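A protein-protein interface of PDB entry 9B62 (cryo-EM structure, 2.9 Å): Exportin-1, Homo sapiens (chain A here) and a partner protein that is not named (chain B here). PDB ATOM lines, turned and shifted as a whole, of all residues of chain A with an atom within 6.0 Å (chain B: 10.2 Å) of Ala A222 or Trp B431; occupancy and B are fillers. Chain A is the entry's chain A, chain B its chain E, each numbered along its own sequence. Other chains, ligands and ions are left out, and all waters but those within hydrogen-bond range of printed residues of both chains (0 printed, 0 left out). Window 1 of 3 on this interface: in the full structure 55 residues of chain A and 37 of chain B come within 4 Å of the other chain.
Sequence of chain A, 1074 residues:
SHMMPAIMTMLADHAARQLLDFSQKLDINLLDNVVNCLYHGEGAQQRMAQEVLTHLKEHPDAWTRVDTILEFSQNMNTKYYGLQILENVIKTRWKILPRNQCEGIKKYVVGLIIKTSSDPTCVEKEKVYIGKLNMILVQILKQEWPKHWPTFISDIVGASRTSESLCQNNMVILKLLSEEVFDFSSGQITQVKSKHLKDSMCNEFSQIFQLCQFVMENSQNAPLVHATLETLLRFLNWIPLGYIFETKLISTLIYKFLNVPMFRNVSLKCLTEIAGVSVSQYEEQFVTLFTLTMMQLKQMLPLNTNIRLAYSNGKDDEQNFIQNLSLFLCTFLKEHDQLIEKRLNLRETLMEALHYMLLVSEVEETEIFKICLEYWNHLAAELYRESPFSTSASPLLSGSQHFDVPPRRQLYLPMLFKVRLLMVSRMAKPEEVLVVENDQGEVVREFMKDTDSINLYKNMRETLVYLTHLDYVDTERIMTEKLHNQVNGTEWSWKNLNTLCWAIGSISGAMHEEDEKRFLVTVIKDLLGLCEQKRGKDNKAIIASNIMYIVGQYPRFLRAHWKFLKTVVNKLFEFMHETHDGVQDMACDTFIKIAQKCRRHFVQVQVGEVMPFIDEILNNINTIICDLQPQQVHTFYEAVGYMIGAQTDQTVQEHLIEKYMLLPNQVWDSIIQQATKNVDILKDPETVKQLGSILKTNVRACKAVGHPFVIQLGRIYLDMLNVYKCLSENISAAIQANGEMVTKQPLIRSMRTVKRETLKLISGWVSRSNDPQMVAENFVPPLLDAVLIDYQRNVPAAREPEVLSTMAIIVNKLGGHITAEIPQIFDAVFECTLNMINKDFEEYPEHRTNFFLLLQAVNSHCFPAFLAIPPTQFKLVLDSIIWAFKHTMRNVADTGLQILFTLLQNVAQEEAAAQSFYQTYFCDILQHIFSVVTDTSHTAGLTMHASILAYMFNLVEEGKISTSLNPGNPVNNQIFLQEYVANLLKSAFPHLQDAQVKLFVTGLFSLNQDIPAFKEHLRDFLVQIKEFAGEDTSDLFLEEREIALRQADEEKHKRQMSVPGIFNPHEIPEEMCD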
ATOM      1  N   SER A 219       1.157 -19.055 -12.642  1.00  0.00           N
ATOM      2  CA  SER A 219       0.310 -20.238 -12.667  1.00  0.00           C
ATOM      3  C   SER A 219       1.131 -21.488 -12.948  1.00  0.00           C
ATOM      4  O   SER A 219       2.064 -21.473 -13.755  1.00  0.00           O
ATOM      5  CB  SER A 219      -0.780 -20.092 -13.723  1.00  0.00           C
ATOM      6  OG  SER A 219      -1.664 -21.196 -13.685  1.00  0.00           O
ATOM      7  N   GLN A 220       0.773 -22.579 -12.269  1.00  0.00           N
ATOM      8  CA  GLN A 220       1.370 -23.890 -12.495  1.00  0.00           C
ATOM      9  C   GLN A 220       0.343 -24.889 -13.011  1.00  0.00           C
ATOM     10  O   GLN A 220       0.578 -26.100 -12.960  1.00  0.00           O
ATOM     11  CB  GLN A 220       2.011 -24.410 -11.209  1.00  0.00           C
ATOM     12  CG  GLN A 220       3.166 -23.562 -10.708  1.00  0.00           C
ATOM     13  CD  GLN A 220       3.724 -24.027  -9.371  1.00  0.00           C
ATOM     14  OE1 GLN A 220       4.637 -23.406  -8.829  1.00  0.00           O
ATOM     15  NE2 GLN A 220       3.183 -25.117  -8.832  1.00  0.00           N
ATOM     16  N   ASN A 221      -0.792 -24.403 -13.504  1.00  0.00           N
ATOM     17  CA  ASN A 221      -1.873 -25.246 -13.992  1.00  0.00           C
ATOM     18  C   ASN A 221      -1.812 -25.278 -15.514  1.00  0.00           C
ATOM     19  O   ASN A 221      -1.965 -24.241 -16.166  1.00  0.00           O
ATOM     20  CB  ASN A 221      -3.220 -24.714 -13.503  1.00  0.00           C
ATOM     21  CG  ASN A 221      -4.371 -25.630 -13.845  1.00  0.00           C
ATOM     22  OD1 ASN A 221      -5.308 -25.234 -14.536  1.00  0.00           O
ATOM     23  ND2 ASN A 221      -4.311 -26.862 -13.360  1.00  0.00           N
ATOM     24  N   ALA A 222      -1.582 -26.464 -16.072  1.00  0.00           N
ATOM     25  CA  ALA A 222      -1.377 -26.573 -17.515  1.00  0.00           C
ATOM     26  C   ALA A 222      -2.573 -26.089 -18.318  1.00  0.00           C
ATOM     27  O   ALA A 222      -2.381 -25.276 -19.238  1.00  0.00           O
ATOM     28  CB  ALA A 222      -1.025 -28.018 -17.872  1.00  0.00           C
ATOM     29  N   PRO A 223      -3.805 -26.540 -18.060  1.00  0.00           N
ATOM     30  CA  PRO A 223      -4.932 -26.035 -18.861  1.00  0.00           C
ATOM     31  C   PRO A 223      -5.131 -24.535 -18.746  1.00  0.00           C
ATOM     32  O   PRO A 223      -5.476 -23.884 -19.739  1.00  0.00           O
ATOM     33  CB  PRO A 223      -6.133 -26.824 -18.316  1.00  0.00           C
ATOM     34  CG  PRO A 223      -5.702 -27.351 -17.002  1.00  0.00           C
ATOM     35  CD  PRO A 223      -4.233 -27.567 -17.095  1.00  0.00           C
ATOM     36  N   LEU A 224      -4.905 -23.956 -17.566  1.00  0.00           N
ATOM     37  CA  LEU A 224      -5.076 -22.517 -17.404  1.00  0.00           C
ATOM     38  C   LEU A 224      -4.069 -21.746 -18.247  1.00  0.00           C
ATOM     39  O   LEU A 224      -4.425 -20.789 -18.947  1.00  0.00           O
ATOM     40  CB  LEU A 224      -4.946 -22.140 -15.929  1.00  0.00           C
ATOM     41  CG  LEU A 224      -4.860 -20.646 -15.618  1.00  0.00           C
ATOM     42  CD1 LEU A 224      -6.005 -19.890 -16.260  1.00  0.00           C
ATOM     43  CD2 LEU A 224      -4.855 -20.421 -14.121  1.00  0.00           C
ATOM     44  N   VAL A 225      -2.799 -22.147 -18.195  1.00  0.00           N
ATOM     45  CA  VAL A 225      -1.777 -21.450 -18.967  1.00  0.00           C
ATOM     46  C   VAL A 225      -2.007 -21.654 -20.457  1.00  0.00           C
ATOM     47  O   VAL A 225      -1.787 -20.744 -21.264  1.00  0.00           O
ATOM     48  CB  VAL A 225      -0.375 -21.918 -18.542  1.00  0.00           C
ATOM     49  CG1 VAL A 225       0.678 -21.254 -19.397  1.00  0.00           C
ATOM     50  CG2 VAL A 225      -0.140 -21.611 -17.078  1.00  0.00           C
ATOM     51  N   HIS A 226      -2.449 -22.849 -20.850  1.00  0.00           N
ATOM     52  CA  HIS A 226      -2.731 -23.084 -22.260  1.00  0.00           C
ATOM     53  C   HIS A 226      -3.883 -22.209 -22.739  1.00  0.00           C
ATOM     54  O   HIS A 226      -3.840 -21.671 -23.849  1.00  0.00           O
ATOM     55  CB  HIS A 226      -3.041 -24.559 -22.501  1.00  0.00           C
ATOM     56  CG  HIS A 226      -2.985 -24.952 -23.942  1.00  0.00           C
ATOM     57  ND1 HIS A 226      -4.100 -24.985 -24.750  1.00  0.00           N
ATOM     58  CD2 HIS A 226      -1.943 -25.318 -24.725  1.00  0.00           C
ATOM     59  CE1 HIS A 226      -3.750 -25.361 -25.966  1.00  0.00           C
ATOM     60  NE2 HIS A 226      -2.446 -25.568 -25.978  1.00  0.00           N
ATOM     61  N   ALA A 227      -4.922 -22.055 -21.916  1.00  0.00           N
ATOM     62  CA  ALA A 227      -6.016 -21.159 -22.272  1.00  0.00           C
ATOM     63  C   ALA A 227      -5.537 -19.717 -22.375  1.00  0.00           C
ATOM     64  O   ALA A 227      -5.945 -18.982 -23.281  1.00  0.00           O
ATOM     65  CB  ALA A 227      -7.142 -21.274 -21.247  1.00  0.00           C
ATOM     66  N   LYS A 256       9.902 -19.735 -21.719  1.00  0.00           N
ATOM     67  CA  LYS A 256       9.076 -20.442 -20.753  1.00  0.00           C
ATOM     68  C   LYS A 256       8.143 -21.456 -21.393  1.00  0.00           C
ATOM     69  O   LYS A 256       7.829 -22.472 -20.763  1.00  0.00           O
ATOM     70  CB  LYS A 256       8.255 -19.445 -19.933  1.00  0.00           C
ATOM     71  CG  LYS A 256       9.102 -18.451 -19.164  1.00  0.00           C
ATOM     72  CD  LYS A 256       8.329 -17.808 -18.025  1.00  0.00           C
ATOM     73  CE  LYS A 256       8.095 -18.789 -16.889  1.00  0.00           C
ATOM     74  NZ  LYS A 256       7.605 -18.110 -15.661  1.00  0.00           N
ATOM     75  N   PHE A 257       7.697 -21.219 -22.624  1.00  0.00           N
ATOM     76  CA  PHE A 257       6.669 -22.049 -23.238  1.00  0.00           C
ATOM     77  C   PHE A 257       7.085 -22.697 -24.546  1.00  0.00           C
ATOM     78  O   PHE A 257       6.553 -23.755 -24.880  1.00  0.00           O
ATOM     79  CB  PHE A 257       5.400 -21.221 -23.481  1.00  0.00           C
ATOM     80  CG  PHE A 257       4.896 -20.525 -22.254  1.00  0.00           C
ATOM     81  CD1 PHE A 257       4.362 -21.248 -21.207  1.00  0.00           C
ATOM     82  CD2 PHE A 257       4.962 -19.152 -22.144  1.00  0.00           C
ATOM     83  CE1 PHE A 257       3.906 -20.616 -20.077  1.00  0.00           C
ATOM     84  CE2 PHE A 257       4.506 -18.517 -21.013  1.00  0.00           C
ATOM     85  CZ  PHE A 257       3.977 -19.252 -19.980  1.00  0.00           C
ATOM     86  N   VAL A 260       8.560 -26.165 -23.838  1.00  0.00           N
ATOM     87  CA  VAL A 260       7.673 -27.157 -23.218  1.00  0.00           C
ATOM     88  C   VAL A 260       6.883 -27.872 -24.311  1.00  0.00           C
ATOM     89  O   VAL A 260       6.242 -27.205 -25.140  1.00  0.00           O
ATOM     90  CB  VAL A 260       6.738 -26.482 -22.217  1.00  0.00           C
ATOM     91  CG1 VAL A 260       5.897 -27.520 -21.500  1.00  0.00           C
ATOM     92  CG2 VAL A 260       7.534 -25.662 -21.220  1.00  0.00           C
ATOM     93  N   MET A 262       4.021 -29.340 -24.463  1.00  0.00           N
ATOM     94  CA  MET A 262       2.589 -29.078 -24.524  1.00  0.00           C
ATOM     95  C   MET A 262       2.262 -27.623 -24.836  1.00  0.00           C
ATOM     96  O   MET A 262       1.080 -27.289 -24.967  1.00  0.00           O
ATOM     97  CB  MET A 262       1.916 -29.487 -23.209  1.00  0.00           C
ATOM     98  CG  MET A 262       2.564 -28.937 -21.955  1.00  0.00           C
ATOM     99  SD  MET A 262       1.624 -29.360 -20.478  1.00  0.00           S
ATOM    100  CE  MET A 262       2.780 -28.894 -19.195  1.00  0.00           C
ATOM    101  N   PHE A 263       3.268 -26.757 -24.963  1.00  0.00           N
ATOM    102  CA  PHE A 263       3.061 -25.360 -25.323  1.00  0.00           C
ATOM    103  C   PHE A 263       3.800 -24.966 -26.596  1.00  0.00           C
ATOM    104  O   PHE A 263       3.851 -23.776 -26.923  1.00  0.00           O
ATOM    105  CB  PHE A 263       3.505 -24.445 -24.177  1.00  0.00           C
ATOM    106  CG  PHE A 263       2.782 -24.688 -22.883  1.00  0.00           C
ATOM    107  CD1 PHE A 263       1.425 -24.941 -22.861  1.00  0.00           C
ATOM    108  CD2 PHE A 263       3.468 -24.657 -21.684  1.00  0.00           C
ATOM    109  CE1 PHE A 263       0.771 -25.160 -21.670  1.00  0.00           C
ATOM    110  CE2 PHE A 263       2.817 -24.875 -20.494  1.00  0.00           C
ATOM    111  CZ  PHE A 263       1.468 -25.126 -20.486  1.00  0.00           C
ATOM    112  N   GLY B 423      -0.821 -20.250  -7.779  1.00  0.00           N
ATOM    113  CA  GLY B 423       0.450 -20.607  -7.189  1.00  0.00           C
ATOM    114  C   GLY B 423       1.415 -19.439  -7.193  1.00  0.00           C
ATOM    115  O   GLY B 423       1.066 -18.294  -7.485  1.00  0.00           O
ATOM    116  N   LYS B 425       4.955 -20.193  -8.308  1.00  0.00           N
ATOM    117  CA  LYS B 425       6.142 -20.773  -8.934  1.00  0.00           C
ATOM    118  C   LYS B 425       7.067 -21.382  -7.875  1.00  0.00           C
ATOM    119  O   LYS B 425       8.180 -20.914  -7.620  1.00  0.00           O
ATOM    120  CB  LYS B 425       6.878 -19.731  -9.784  1.00  0.00           C
ATOM    121  CG  LYS B 425       6.187 -19.409 -11.097  1.00  0.00           C
ATOM    122  CD  LYS B 425       6.213 -20.592 -12.056  1.00  0.00           C
ATOM    123  CE  LYS B 425       5.510 -20.264 -13.361  1.00  0.00           C
ATOM    124  NZ  LYS B 425       5.523 -21.413 -14.306  1.00  0.00           N
ATOM    125  N   ASP B 426       6.554 -22.443  -7.253  1.00  0.00           N
ATOM    126  CA  ASP B 426       7.293 -23.142  -6.211  1.00  0.00           C
ATOM    127  C   ASP B 426       8.722 -23.419  -6.660  1.00  0.00           C
ATOM    128  O   ASP B 426       9.006 -23.565  -7.851  1.00  0.00           O
ATOM    129  CB  ASP B 426       6.593 -24.456  -5.858  1.00  0.00           C
ATOM    130  CG  ASP B 426       5.164 -24.248  -5.399  1.00  0.00           C
ATOM    131  OD1 ASP B 426       4.339 -23.785  -6.214  1.00  0.00           O
ATOM    132  OD2 ASP B 426       4.863 -24.548  -4.225  1.00  0.00           O
ATOM    133  N   LYS B 427       9.625 -23.489  -5.687  1.00  0.00           N
ATOM    134  CA  LYS B 427      11.039 -23.655  -5.989  1.00  0.00           C
ATOM    135  C   LYS B 427      11.274 -24.917  -6.811  1.00  0.00           C
ATOM    136  O   LYS B 427      10.700 -25.975  -6.541  1.00  0.00           O
ATOM    137  CB  LYS B 427      11.855 -23.709  -4.693  1.00  0.00           C
ATOM    138  CG  LYS B 427      11.790 -25.034  -3.929  1.00  0.00           C
ATOM    139  CD  LYS B 427      10.372 -25.397  -3.514  1.00  0.00           C
ATOM    140  CE  LYS B 427      10.350 -26.648  -2.651  1.00  0.00           C
ATOM    141  NZ  LYS B 427       8.965 -27.031  -2.261  1.00  0.00           N
ATOM    142  N   ASN B 428      12.130 -24.794  -7.825  1.00  0.00           N
ATOM    143  CA  ASN B 428      12.542 -25.928  -8.650  1.00  0.00           C
ATOM    144  C   ASN B 428      11.337 -26.615  -9.289  1.00  0.00           C
ATOM    145  O   ASN B 428      11.174 -27.835  -9.214  1.00  0.00           O
ATOM    146  CB  ASN B 428      13.364 -26.922  -7.826  1.00  0.00           C
ATOM    147  CG  ASN B 428      14.571 -26.279  -7.176  1.00  0.00           C
ATOM    148  OD1 ASN B 428      14.651 -25.056  -7.066  1.00  0.00           O
ATOM    149  ND2 ASN B 428      15.516 -27.102  -6.738  1.00  0.00           N
ATOM    150  N   PHE B 429      10.485 -25.817  -9.926  1.00  0.00           N
ATOM    151  CA  PHE B 429       9.345 -26.321 -10.679  1.00  0.00           C
ATOM    152  C   PHE B 429       9.595 -26.123 -12.167  1.00  0.00           C
ATOM    153  O   PHE B 429       9.974 -25.028 -12.597  1.00  0.00           O
ATOM    154  CB  PHE B 429       8.050 -25.616 -10.278  1.00  0.00           C
ATOM    155  CG  PHE B 429       6.900 -25.902 -11.203  1.00  0.00           C
ATOM    156  CD1 PHE B 429       6.111 -27.024 -11.021  1.00  0.00           C
ATOM    157  CD2 PHE B 429       6.614 -25.055 -12.260  1.00  0.00           C
ATOM    158  CE1 PHE B 429       5.059 -27.292 -11.871  1.00  0.00           C
ATOM    159  CE2 PHE B 429       5.565 -25.320 -13.113  1.00  0.00           C
ATOM    160  CZ  PHE B 429       4.786 -26.440 -12.918  1.00  0.00           C
ATOM    161  N   GLN B 430       9.384 -27.181 -12.943  1.00  0.00           N
ATOM    162  CA  GLN B 430       9.454 -27.106 -14.392  1.00  0.00           C
ATOM    163  C   GLN B 430       8.331 -27.947 -14.979  1.00  0.00           C
ATOM    164  O   GLN B 430       7.933 -28.964 -14.406  1.00  0.00           O
ATOM    165  CB  GLN B 430      10.809 -27.589 -14.922  1.00  0.00           C
ATOM    166  CG  GLN B 430      11.128 -29.039 -14.597  1.00  0.00           C
ATOM    167  CD  GLN B 430      12.391 -29.522 -15.276  1.00  0.00           C
ATOM    168  OE1 GLN B 430      12.433 -30.623 -15.824  1.00  0.00           O
ATOM    169  NE2 GLN B 430      13.434 -28.699 -15.246  1.00  0.00           N
ATOM    170  N   TRP B 431       7.824 -27.514 -16.127  1.00  0.00           N
ATOM    171  CA  TRP B 431       6.755 -28.247 -16.778  1.00  0.00           C
ATOM    172  C   TRP B 431       7.250 -29.618 -17.223  1.00  0.00           C
ATOM    173  O   TRP B 431       8.448 -29.845 -17.413  1.00  0.00           O
ATOM    174  CB  TRP B 431       6.218 -27.464 -17.975  1.00  0.00           C
ATOM    175  CG  TRP B 431       5.707 -26.105 -17.617  1.00  0.00           C
ATOM    176  CD1 TRP B 431       6.397 -24.933 -17.666  1.00  0.00           C
ATOM    177  CD2 TRP B 431       4.392 -25.778 -17.155  1.00  0.00           C
ATOM    178  NE1 TRP B 431       5.596 -23.894 -17.263  1.00  0.00           N
ATOM    179  CE2 TRP B 431       4.359 -24.387 -16.945  1.00  0.00           C
ATOM    180  CE3 TRP B 431       3.241 -26.526 -16.900  1.00  0.00           C
ATOM    181  CZ2 TRP B 431       3.221 -23.730 -16.491  1.00  0.00           C
ATOM    182  CZ3 TRP B 431       2.112 -25.870 -16.452  1.00  0.00           C
ATOM    183  CH2 TRP B 431       2.110 -24.488 -16.251  1.00  0.00           C
ATOM    184  N   ALA B 432       6.309 -30.544 -17.379  1.00  0.00           N
ATOM    185  CA  ALA B 432       6.662 -31.900 -17.769  1.00  0.00           C
ATOM    186  C   ALA B 432       7.368 -31.901 -19.118  1.00  0.00           C
ATOM    187  O   ALA B 432       6.921 -31.253 -20.068  1.00  0.00           O
ATOM    188  CB  ALA B 432       5.410 -32.774 -17.827  1.00  0.00           C
ATOM    189  N   ASN B 433       8.478 -32.635 -19.196  1.00  0.00           N
ATOM    190  CA  ASN B 433       9.224 -32.810 -20.441  1.00  0.00           C
ATOM    191  C   ASN B 433       9.796 -31.494 -20.960  1.00  0.00           C
ATOM    192  O   ASN B 433       9.935 -31.303 -22.169  1.00  0.00           O
ATOM    193  CB  ASN B 433       8.347 -33.459 -21.515  1.00  0.00           C
ATOM    194  CG  ASN B 433       7.804 -34.803 -21.089  1.00  0.00           C
ATOM    195  OD1 ASN B 433       7.972 -35.219 -19.943  1.00  0.00           O
ATOM    196  ND2 ASN B 433       7.142 -35.491 -22.010  1.00  0.00           N
ATOM    197  N   THR B 434      10.144 -30.578 -20.058  1.00  0.00           N
ATOM    198  CA  THR B 434      10.717 -29.303 -20.471  1.00  0.00           C
ATOM    199  C   THR B 434      12.035 -29.517 -21.204  1.00  0.00           C
ATOM    200  O   THR B 434      13.016 -29.973 -20.608  1.00  0.00           O
ATOM    201  CB  THR B 434      10.934 -28.391 -19.264  1.00  0.00           C
ATOM    202  OG1 THR B 434       9.670 -28.048 -18.688  1.00  0.00           O
ATOM    203  CG2 THR B 434      11.660 -27.122 -19.675  1.00  0.00           C
ATOM    204  N   GLY B 435      12.066 -29.190 -22.493  1.00  0.00           N
ATOM    205  CA  GLY B 435      13.269 -29.298 -23.290  1.00  0.00           C
ATOM    206  C   GLY B 435      13.363 -30.538 -24.149  1.00  0.00           C
ATOM    207  O   GLY B 435      14.386 -30.728 -24.818  1.00  0.00           O
ATOM    208  N   ALA B 436      12.337 -31.382 -24.161  1.00  0.00           N
ATOM    209  CA  ALA B 436      12.385 -32.604 -24.949  1.00  0.00           C
ATOM    210  C   ALA B 436      12.441 -32.285 -26.438  1.00  0.00           C
ATOM    211  O   ALA B 436      11.893 -31.283 -26.904  1.00  0.00           O
ATOM    212  CB  ALA B 436      11.170 -33.480 -24.650  1.00  0.00           C
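The side-chain amide oxygen (OE1) of Gln A220 lies close to the backbone NH (N) of Lys B425 (3.3 Å).
OE1 of Gln A220 lies close to OD1 of Asp B426, at 2.7 Å.
The side-chain hydroxyl (OG) of Ser A219 sits at hydrogen-bond distance from the backbone NH (N) of Asn A221, at 3.3 Å.
OD1 of Asn A221 sits at hydrogen-bond distance from N of Leu A224, 3.3 Å away.
O of Trp B431 lies within hydrogen-bond range of OG1 of Thr B434.
Ser A219 touches Lys B425 (O to NZ, 3.5 Å).
Trp B431 touches Ser A219.
CG of Gln A220 touches CE2 of Phe B429 (3.8 Å).
Trp B431 touches Gln A220 (CH2 to C, 3.7 Å).
Asn A221 touches Trp B431.
Trp B431 touches Ala A222.
CG2 of Val A225 touches CH2 of Trp B431, at 3.7 Å.
Trp B431 touches Val A260 (CB to CG1, 3.5 Å).
Met A262 touches Trp B431 (CE to CE3, 3.3 Å).
CD2 of Trp B431 touches CE2 of Phe A263, at 3.8 Å.
Printed residues of chain B within 4 Å of Asn A221: Trp B431 (3.997 Å).
Of chain B, only Trp B431 (3.7 Å) comes within 4 Å of Ala A222.
No residue of chain B comes within 4 Å of Pro A223.
Val A225 touches just one residue of chain B: Trp B431.
His A226 touches none of the printed residues of chain B.
Of the printed residues of chain A, Lys B425 touches Ser A219, Gln A220 and Lys A256.
Of the printed residues of chain A, Phe B429 touches Gln A220.
Ala B436 touches none of the printed residues of chain A.
The nearest residue of chain B that does not touch Ala A222 is Phe B429 (7.1 Å).
Of the 13 printed residues of chain B, 4 touch a printed residue of chain A.
Hydrophobic or aromatic side chains of chain B within 4 Å of the printed part of chain A: Phe B429 and Trp B431.
Of the 14 printed residues of chain A, 9 touch a printed residue of chain B.
Printed residues of chain A that touch a printed residue of chain B: Ser A219, Gln A220, Asn A221, Ala A222, Val A225, Lys A256, Val A260, Met A262 and Phe A263.
Among the printed residues, 13 pairs touch across the chains.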
